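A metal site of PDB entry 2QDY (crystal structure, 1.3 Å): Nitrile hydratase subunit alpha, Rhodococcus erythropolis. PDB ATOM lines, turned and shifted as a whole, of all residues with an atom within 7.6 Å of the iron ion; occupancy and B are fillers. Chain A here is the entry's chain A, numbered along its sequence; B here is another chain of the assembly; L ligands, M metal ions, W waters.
NH2 of Arg 141 of chain B lies within salt-bridge range of OD2 of CSD 115 (2.9 Å). O of CSD 115 is in hydrogen-bond range of the side-chain hydroxyl (OH) of Tyr 128, at 2.8 Å. OG1 of Thr 116 is in hydrogen-bond range of O of Ser 114. OH of Tyr 72 of chain B sits at hydrogen-bond distance from OG of Ser 114, at 2.6 Å. OD1 of CSD 113 is in salt-bridge range of the guanidinium group (NH1) of Arg 141 of chain B (2.9 Å). NE of Arg 56 of chain B lies within salt-bridge range of OD2 of CSD 113 (2.9 Å). O of Thr 163 sits close to SG of Cys 110 (3.5 Å). N of Cys 110 is in hydrogen-bond range of OH of Tyr 128 (3.5 Å).
A nitrogen (N1) of the ligand lies within hydrogen-bond range of the side-chain hydroxyl (OH) of Tyr 72 of chain B.
The iron ion is bound by N of CSD 115, at 2.0 Å. N of Ser 114 binds the iron ion (2.0 Å). The iron ion is bound by water W1, 2.1 Å away. SG of CSD 113 is bound to the iron ion (2.2 Å). The iron ion is bound by SG of CSD 115 (2.2 Å). The iron ion is bound by SG of Cys 110, at 2.2 Å. The iron ion has six donor atoms within binding distance.
Of the 23 residues printed, 4 come within 4 Å of the iron ion.
Water W1 lies within hydrogen-bond range of the side-chain hydroxyl of Ser 114, OD1 of CSD 115 and OD2 of CSD 113.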
ATOM      1  N   GLN A  91      -2.503  -3.519  15.366  1.00  0.00           N
ATOM      2  CA  GLN A  91      -2.338  -4.864  15.914  1.00  0.00           C
ATOM      3  C   GLN A  91      -0.897  -5.048  16.358  1.00  0.00           C
ATOM      4  O   GLN A  91      -0.340  -6.131  16.308  1.00  0.00           O
ATOM      5  CB  GLN A  91      -2.782  -5.951  14.916  1.00  0.00           C
ATOM      6  CG  GLN A  91      -4.262  -5.831  14.581  1.00  0.00           C
ATOM      7  CD  GLN A  91      -5.086  -6.173  15.783  1.00  0.00           C
ATOM      8  OE1 GLN A  91      -4.846  -7.219  16.390  1.00  0.00           O
ATOM      9  NE2 GLN A  91      -5.986  -5.297  16.169  1.00  0.00           N
ATOM     10  N   VAL A 109      -0.054 -18.187  19.657  1.00  0.00           N
ATOM     11  CA  VAL A 109      -1.249 -18.535  18.849  1.00  0.00           C
ATOM     12  C   VAL A 109      -2.342 -17.473  19.141  1.00  0.00           C
ATOM     13  O   VAL A 109      -2.259 -16.766  20.172  1.00  0.00           O
ATOM     14  CB  VAL A 109      -1.752 -19.986  19.196  1.00  0.00           C
ATOM     15  CG1 VAL A 109      -2.219 -20.013  20.672  1.00  0.00           C
ATOM     16  CG2 VAL A 109      -2.913 -20.401  18.285  1.00  0.00           C
ATOM     17  N   CYS A 110      -3.350 -17.441  18.283  1.00  0.00           N
ATOM     18  CA  CYS A 110      -4.610 -16.818  18.646  1.00  0.00           C
ATOM     19  C   CYS A 110      -5.677 -17.905  18.457  1.00  0.00           C
ATOM     20  O   CYS A 110      -6.177 -18.133  17.341  1.00  0.00           O
ATOM     21  CB  CYS A 110      -4.893 -15.654  17.737  1.00  0.00           C
ATOM     22  SG  CYS A 110      -6.493 -14.822  18.116  1.00  0.00           S
ATOM     23  N   SER A 111      -6.010 -18.598  19.548  1.00  0.00           N
ATOM     24  CA  SER A 111      -6.922 -19.721  19.401  1.00  0.00           C
ATOM     25  C   SER A 111      -8.296 -19.271  18.957  1.00  0.00           C
ATOM     26  O   SER A 111      -9.021 -20.037  18.296  1.00  0.00           O
ATOM     27  CB  SER A 111      -7.027 -20.568  20.680  1.00  0.00           C
ATOM     28  OG  SER A 111      -7.724 -19.853  21.692  1.00  0.00           O
ATOM     29  N   LEU A 112      -8.680 -18.024  19.260  1.00  0.00           N
ATOM     30  CA  LEU A 112     -10.024 -17.557  18.974  1.00  0.00           C
ATOM     31  C   LEU A 112     -10.172 -16.955  17.556  1.00  0.00           C
ATOM     32  O   LEU A 112     -11.304 -16.726  17.140  1.00  0.00           O
ATOM     33  CB  LEU A 112     -10.472 -16.531  20.051  1.00  0.00           C
ATOM     34  CG  LEU A 112     -10.557 -17.132  21.459  1.00  0.00           C
ATOM     35  CD1 LEU A 112     -10.683 -15.995  22.480  1.00  0.00           C
ATOM     36  CD2 LEU A 112     -11.762 -18.075  21.616  1.00  0.00           C
ATOM     37  N   CSD A 113      -9.047 -16.725  16.863  1.00  0.00           N
ATOM     38  CA  CSD A 113      -9.072 -16.095  15.529  1.00  0.00           C
ATOM     39  CB  CSD A 113      -9.801 -14.682  15.588  1.00  0.00           C
ATOM     40  SG  CSD A 113      -9.083 -13.538  16.809  1.00  0.00           S
ATOM     41  C   CSD A 113      -7.701 -16.066  14.873  1.00  0.00           C
ATOM     42  O   CSD A 113      -7.395 -17.029  14.145  1.00  0.00           O
ATOM     43  OD1 CSD A 113      -9.523 -14.063  18.171  1.00  0.00           O
ATOM     44  OD2 CSD A 113      -9.808 -12.263  16.490  1.00  0.00           O
ATOM     45  N   SER A 114      -6.878 -14.997  15.055  1.00  0.00           N
ATOM     46  CA  SER A 114      -5.634 -14.987  14.285  1.00  0.00           C
ATOM     47  C   SER A 114      -4.682 -13.920  14.773  1.00  0.00           C
ATOM     48  O   SER A 114      -3.607 -13.704  14.158  1.00  0.00           O
ATOM     49  CB  SER A 114      -5.897 -14.702  12.824  1.00  0.00           C
ATOM     50  OG  SER A 114      -6.329 -13.346  12.634  1.00  0.00           O
ATOM     51  N   CSD A 115      -5.059 -13.278  15.866  1.00  0.00           N
ATOM     52  CA  CSD A 115      -4.280 -12.160  16.395  1.00  0.00           C
ATOM     53  CB  CSD A 115      -4.817 -11.767  17.772  1.00  0.00           C
ATOM     54  SG  CSD A 115      -6.634 -11.682  17.583  1.00  0.00           S
ATOM     55  C   CSD A 115      -2.785 -12.455  16.452  1.00  0.00           C
ATOM     56  O   CSD A 115      -2.295 -13.488  16.955  1.00  0.00           O
ATOM     57  OD1 CSD A 115      -6.858 -10.420  16.693  1.00  0.00           O
ATOM     58  OD2 CSD A 115      -7.217 -11.489  18.924  1.00  0.00           O
ATOM     59  N   THR A 116      -2.052 -11.423  15.961  1.00  0.00           N
ATOM     60  CA  THR A 116      -0.615 -11.502  15.624  1.00  0.00           C
ATOM     61  C   THR A 116      -0.100 -10.062  15.689  1.00  0.00           C
ATOM     62  O   THR A 116      -0.825  -9.151  15.303  1.00  0.00           O
ATOM     63  CB  THR A 116      -0.529 -11.948  14.146  1.00  0.00           C
ATOM     64  OG1 THR A 116      -0.914 -13.336  14.051  1.00  0.00           O
ATOM     65  CG2 THR A 116       0.869 -11.796  13.563  1.00  0.00           C
ATOM     66  N   TRP A 118       1.153  -7.785  13.898  1.00  0.00           N
ATOM     67  CA  TRP A 118       1.310  -7.562  12.435  1.00  0.00           C
ATOM     68  C   TRP A 118       2.555  -6.753  12.016  1.00  0.00           C
ATOM     69  O   TRP A 118       3.209  -7.122  11.067  1.00  0.00           O
ATOM     70  CB  TRP A 118       0.119  -6.806  11.874  1.00  0.00           C
ATOM     71  CG  TRP A 118      -1.173  -7.544  11.812  1.00  0.00           C
ATOM     72  CD1 TRP A 118      -1.397  -8.897  12.007  1.00  0.00           C
ATOM     73  CD2 TRP A 118      -2.435  -6.954  11.479  1.00  0.00           C
ATOM     74  NE1 TRP A 118      -2.764  -9.167  11.794  1.00  0.00           N
ATOM     75  CE2 TRP A 118      -3.414  -7.996  11.479  1.00  0.00           C
ATOM     76  CE3 TRP A 118      -2.832  -5.644  11.186  1.00  0.00           C
ATOM     77  CZ2 TRP A 118      -4.751  -7.751  11.180  1.00  0.00           C
ATOM     78  CZ3 TRP A 118      -4.176  -5.388  10.908  1.00  0.00           C
ATOM     79  CH2 TRP A 118      -5.118  -6.433  10.882  1.00  0.00           C
ATOM     80  N   PRO A 124      -0.563 -12.839   9.665  1.00  0.00           N
ATOM     81  CA  PRO A 124      -0.339 -14.272   9.926  1.00  0.00           C
ATOM     82  C   PRO A 124      -0.461 -15.098   8.643  1.00  0.00           C
ATOM     83  O   PRO A 124      -1.234 -14.770   7.752  1.00  0.00           O
ATOM     84  CB  PRO A 124      -1.488 -14.639  10.889  1.00  0.00           C
ATOM     85  CG  PRO A 124      -2.531 -13.562  10.700  1.00  0.00           C
ATOM     86  CD  PRO A 124      -1.733 -12.295  10.372  1.00  0.00           C
ATOM     87  N   TYR A 128      -1.160 -20.529  10.489  1.00  0.00           N
ATOM     88  CA  TYR A 128      -1.331 -20.064  11.856  1.00  0.00           C
ATOM     89  C   TYR A 128      -2.803 -19.824  12.161  1.00  0.00           C
ATOM     90  O   TYR A 128      -3.224 -19.918  13.320  1.00  0.00           O
ATOM     91  CB  TYR A 128      -0.500 -18.777  12.007  1.00  0.00           C
ATOM     92  CG  TYR A 128      -0.622 -18.027  13.315  1.00  0.00           C
ATOM     93  CD1 TYR A 128      -1.621 -17.064  13.518  1.00  0.00           C
ATOM     94  CD2 TYR A 128       0.323 -18.209  14.298  1.00  0.00           C
ATOM     95  CE1 TYR A 128      -1.682 -16.344  14.678  1.00  0.00           C
ATOM     96  CE2 TYR A 128       0.255 -17.498  15.490  1.00  0.00           C
ATOM     97  CZ  TYR A 128      -0.729 -16.537  15.651  1.00  0.00           C
ATOM     98  OH  TYR A 128      -0.689 -15.774  16.796  1.00  0.00           O
ATOM     99  N   LYS A 129      -3.562 -19.453  11.125  1.00  0.00           N
ATOM    100  CA  LYS A 129      -4.976 -19.214  11.251  1.00  0.00           C
ATOM    101  C   LYS A 129      -5.802 -20.475  11.047  1.00  0.00           C
ATOM    102  O   LYS A 129      -7.022 -20.419  11.114  1.00  0.00           O
ATOM    103  CB  LYS A 129      -5.418 -18.160  10.176  1.00  0.00           C
ATOM    104  CG  LYS A 129      -4.731 -16.866  10.306  1.00  0.00           C
ATOM    105  CD  LYS A 129      -5.058 -15.911   9.149  1.00  0.00           C
ATOM    106  CE  LYS A 129      -4.430 -16.207   7.807  1.00  0.00           C
ATOM    107  NZ  LYS A 129      -4.309 -14.971   6.943  1.00  0.00           N
ATOM    108  N   ARG A 134      -4.957 -23.616  15.697  1.00  0.00           N
ATOM    109  CA  ARG A 134      -5.756 -23.014  16.756  1.00  0.00           C
ATOM    110  C   ARG A 134      -6.286 -24.011  17.785  1.00  0.00           C
ATOM    111  O   ARG A 134      -6.388 -23.699  18.967  1.00  0.00           O
ATOM    112  CB  ARG A 134      -6.915 -22.263  16.121  1.00  0.00           C
ATOM    113  CG  ARG A 134      -6.455 -21.008  15.374  1.00  0.00           C
ATOM    114  CD  ARG A 134      -7.553 -20.286  14.611  1.00  0.00           C
ATOM    115  NE  ARG A 134      -8.710 -20.046  15.470  1.00  0.00           N
ATOM    116  CZ  ARG A 134      -9.975 -19.880  15.064  1.00  0.00           C
ATOM    117  NH1 ARG A 134     -10.282 -19.816  13.759  1.00  0.00           N
ATOM    118  NH2 ARG A 134     -10.967 -19.846  15.971  1.00  0.00           N
ATOM    119  N   ASP A 162      -1.590 -17.505  24.353  1.00  0.00           N
ATOM    120  CA  ASP A 162      -2.806 -17.361  23.548  1.00  0.00           C
ATOM    121  C   ASP A 162      -3.128 -15.881  23.531  1.00  0.00           C
ATOM    122  O   ASP A 162      -3.359 -15.268  24.596  1.00  0.00           O
ATOM    123  CB  ASP A 162      -3.926 -18.206  24.174  1.00  0.00           C
ATOM    124  CG  ASP A 162      -5.072 -18.453  23.224  1.00  0.00           C
ATOM    125  OD1 ASP A 162      -5.105 -17.820  22.143  1.00  0.00           O
ATOM    126  OD2 ASP A 162      -5.969 -19.251  23.597  1.00  0.00           O
ATOM    127  N   THR A 163      -3.159 -15.315  22.331  1.00  0.00           N
ATOM    128  CA  THR A 163      -3.335 -13.862  22.123  1.00  0.00           C
ATOM    129  C   THR A 163      -4.833 -13.561  22.197  1.00  0.00           C
ATOM    130  O   THR A 163      -5.529 -13.544  21.178  1.00  0.00           O
ATOM    131  CB  THR A 163      -2.729 -13.476  20.776  1.00  0.00           C
ATOM    132  OG1 THR A 163      -1.361 -13.940  20.706  1.00  0.00           O
ATOM    133  CG2 THR A 163      -2.740 -11.971  20.575  1.00  0.00           C
ATOM    134  N   THR A 164      -5.331 -13.328  23.404  1.00  0.00           N
ATOM    135  CA  THR A 164      -6.753 -13.202  23.677  1.00  0.00           C
ATOM    136  C   THR A 164      -7.180 -11.774  23.957  1.00  0.00           C
ATOM    137  O   THR A 164      -8.376 -11.548  24.055  1.00  0.00           O
ATOM    138  CB  THR A 164      -7.145 -14.098  24.865  1.00  0.00           C
ATOM    139  OG1 THR A 164      -6.216 -13.895  25.946  1.00  0.00           O
ATOM    140  CG2 THR A 164      -7.089 -15.573  24.473  1.00  0.00           C
ATOM    141  N   ARG A 168       0.365  -7.997  22.126  1.00  0.00           N
ATOM    142  CA  ARG A 168       0.849  -8.631  20.917  1.00  0.00           C
ATOM    143  C   ARG A 168       2.258  -9.073  21.153  1.00  0.00           C
ATOM    144  O   ARG A 168       3.093  -8.320  21.649  1.00  0.00           O
ATOM    145  CB  ARG A 168       0.718  -7.688  19.715  1.00  0.00           C
ATOM    146  CG  ARG A 168      -0.725  -7.391  19.358  1.00  0.00           C
ATOM    147  CD  ARG A 168      -1.416  -8.541  18.667  1.00  0.00           C
ATOM    148  NE  ARG A 168      -2.835  -8.279  18.429  1.00  0.00           N
ATOM    149  CZ  ARG A 168      -3.800  -8.346  19.356  1.00  0.00           C
ATOM    150  NH1 ARG A 168      -3.513  -8.753  20.587  1.00  0.00           N
ATOM    151  NH2 ARG A 168      -5.064  -8.035  19.046  1.00  0.00           N
ATOM    152  N   TYR B  37      -9.748  -6.803   5.460  1.00  0.00           N
ATOM    153  CA  TYR B  37      -9.111  -6.024   6.525  1.00  0.00           C
ATOM    154  C   TYR B  37      -9.188  -4.531   6.202  1.00  0.00           C
ATOM    155  O   TYR B  37      -9.398  -3.706   7.105  1.00  0.00           O
ATOM    156  CB  TYR B  37      -7.615  -6.393   6.697  1.00  0.00           C
ATOM    157  CG  TYR B  37      -7.297  -7.719   7.405  1.00  0.00           C
ATOM    158  CD1 TYR B  37      -8.279  -8.586   7.933  1.00  0.00           C
ATOM    159  CD2 TYR B  37      -5.973  -8.050   7.558  1.00  0.00           C
ATOM    160  CE1 TYR B  37      -7.902  -9.755   8.627  1.00  0.00           C
ATOM    161  CE2 TYR B  37      -5.594  -9.189   8.261  1.00  0.00           C
ATOM    162  CZ  TYR B  37      -6.552 -10.007   8.793  1.00  0.00           C
ATOM    163  OH  TYR B  37      -6.143 -11.118   9.481  1.00  0.00           O
ATOM    164  N   ARG B  56     -14.805  -9.155  15.517  1.00  0.00           N
ATOM    165  CA  ARG B  56     -14.594 -10.515  16.039  1.00  0.00           C
ATOM    166  C   ARG B  56     -15.919 -11.185  16.321  1.00  0.00           C
ATOM    167  O   ARG B  56     -16.126 -12.375  15.952  1.00  0.00           O
ATOM    168  CB  ARG B  56     -13.782 -10.496  17.314  1.00  0.00           C
ATOM    169  CG  ARG B  56     -12.364  -9.967  17.106  1.00  0.00           C
ATOM    170  CD  ARG B  56     -11.491 -10.345  18.329  1.00  0.00           C
ATOM    171  NE  ARG B  56     -10.110  -9.895  18.109  1.00  0.00           N
ATOM    172  CZ  ARG B  56      -9.652  -8.673  18.373  1.00  0.00           C
ATOM    173  NH1 ARG B  56     -10.468  -7.819  19.021  1.00  0.00           N
ATOM    174  NH2 ARG B  56      -8.411  -8.344  17.984  1.00  0.00           N
ATOM    175  N   TYR B  72     -10.507 -18.368   5.978  1.00  0.00           N
ATOM    176  CA  TYR B  72     -10.286 -17.225   6.861  1.00  0.00           C
ATOM    177  C   TYR B  72     -10.697 -15.858   6.285  1.00  0.00           C
ATOM    178  O   TYR B  72     -11.523 -15.196   6.861  1.00  0.00           O
ATOM    179  CB  TYR B  72      -8.782 -17.194   7.238  1.00  0.00           C
ATOM    180  CG  TYR B  72      -8.440 -16.027   8.115  1.00  0.00           C
ATOM    181  CD1 TYR B  72      -8.640 -16.073   9.475  1.00  0.00           C
ATOM    182  CD2 TYR B  72      -8.028 -14.812   7.557  1.00  0.00           C
ATOM    183  CE1 TYR B  72      -8.383 -14.995  10.286  1.00  0.00           C
ATOM    184  CE2 TYR B  72      -7.747 -13.685   8.373  1.00  0.00           C
ATOM    185  CZ  TYR B  72      -7.935 -13.803   9.704  1.00  0.00           C
ATOM    186  OH  TYR B  72      -7.688 -12.734  10.517  1.00  0.00           O
ATOM    187  N   TYR B  76     -14.152 -12.795   7.099  1.00  0.00           N
ATOM    188  CA  TYR B  76     -14.155 -11.329   7.363  1.00  0.00           C
ATOM    189  C   TYR B  76     -14.918 -10.569   6.282  1.00  0.00           C
ATOM    190  O   TYR B  76     -15.472  -9.523   6.605  1.00  0.00           O
ATOM    191  CB  TYR B  76     -12.694 -10.832   7.585  1.00  0.00           C
ATOM    192  CG  TYR B  76     -12.190 -11.439   8.866  1.00  0.00           C
ATOM    193  CD1 TYR B  76     -12.443 -10.847  10.086  1.00  0.00           C
ATOM    194  CD2 TYR B  76     -11.628 -12.701   8.853  1.00  0.00           C
ATOM    195  CE1 TYR B  76     -12.060 -11.500  11.304  1.00  0.00           C
ATOM    196  CE2 TYR B  76     -11.294 -13.326   9.995  1.00  0.00           C
ATOM    197  CZ  TYR B  76     -11.495 -12.746  11.230  1.00  0.00           C
ATOM    198  OH  TYR B  76     -11.108 -13.474  12.359  1.00  0.00           O
ATOM    199  N   ARG B 141     -13.697 -12.574  25.614  1.00  0.00           N
ATOM    200  CA  ARG B 141     -12.319 -12.912  25.255  1.00  0.00           C
ATOM    201  C   ARG B 141     -11.699 -13.859  26.251  1.00  0.00           C
ATOM    202  O   ARG B 141     -10.540 -13.759  26.660  1.00  0.00           O
ATOM    203  CB  ARG B 141     -11.462 -11.642  25.070  1.00  0.00           C
ATOM    204  CG  ARG B 141     -11.913 -10.814  23.865  1.00  0.00           C
ATOM    205  CD  ARG B 141     -11.887 -11.619  22.551  1.00  0.00           C
ATOM    206  NE  ARG B 141     -10.529 -12.064  22.239  1.00  0.00           N
ATOM    207  CZ  ARG B 141     -10.249 -12.684  21.087  1.00  0.00           C
ATOM    208  NH1 ARG B 141     -11.236 -13.182  20.308  1.00  0.00           N
ATOM    209  NH2 ARG B 141      -8.981 -12.886  20.747  1.00  0.00           N
HETATM  210  C1  LIG L   1      -7.925  -7.753  13.425  1.00  0.00           C
HETATM  211  C2  LIG L   1      -9.063  -8.634  13.065  1.00  0.00           C
HETATM  212  C3  LIG L   1      -9.626  -9.182  14.423  1.00  0.00           C
HETATM  213  C4  LIG L   1      -8.206  -9.647  12.489  1.00  0.00           C
HETATM  214  N1  LIG L   1      -8.915 -10.585  12.024  1.00  0.00           N
HETATM  215 FE    FE M   1      -6.952 -13.486  16.396  1.00  0.00          FE
HETATM  216  O   HOH W   1      -7.460 -12.348  14.691  1.00  0.00           O
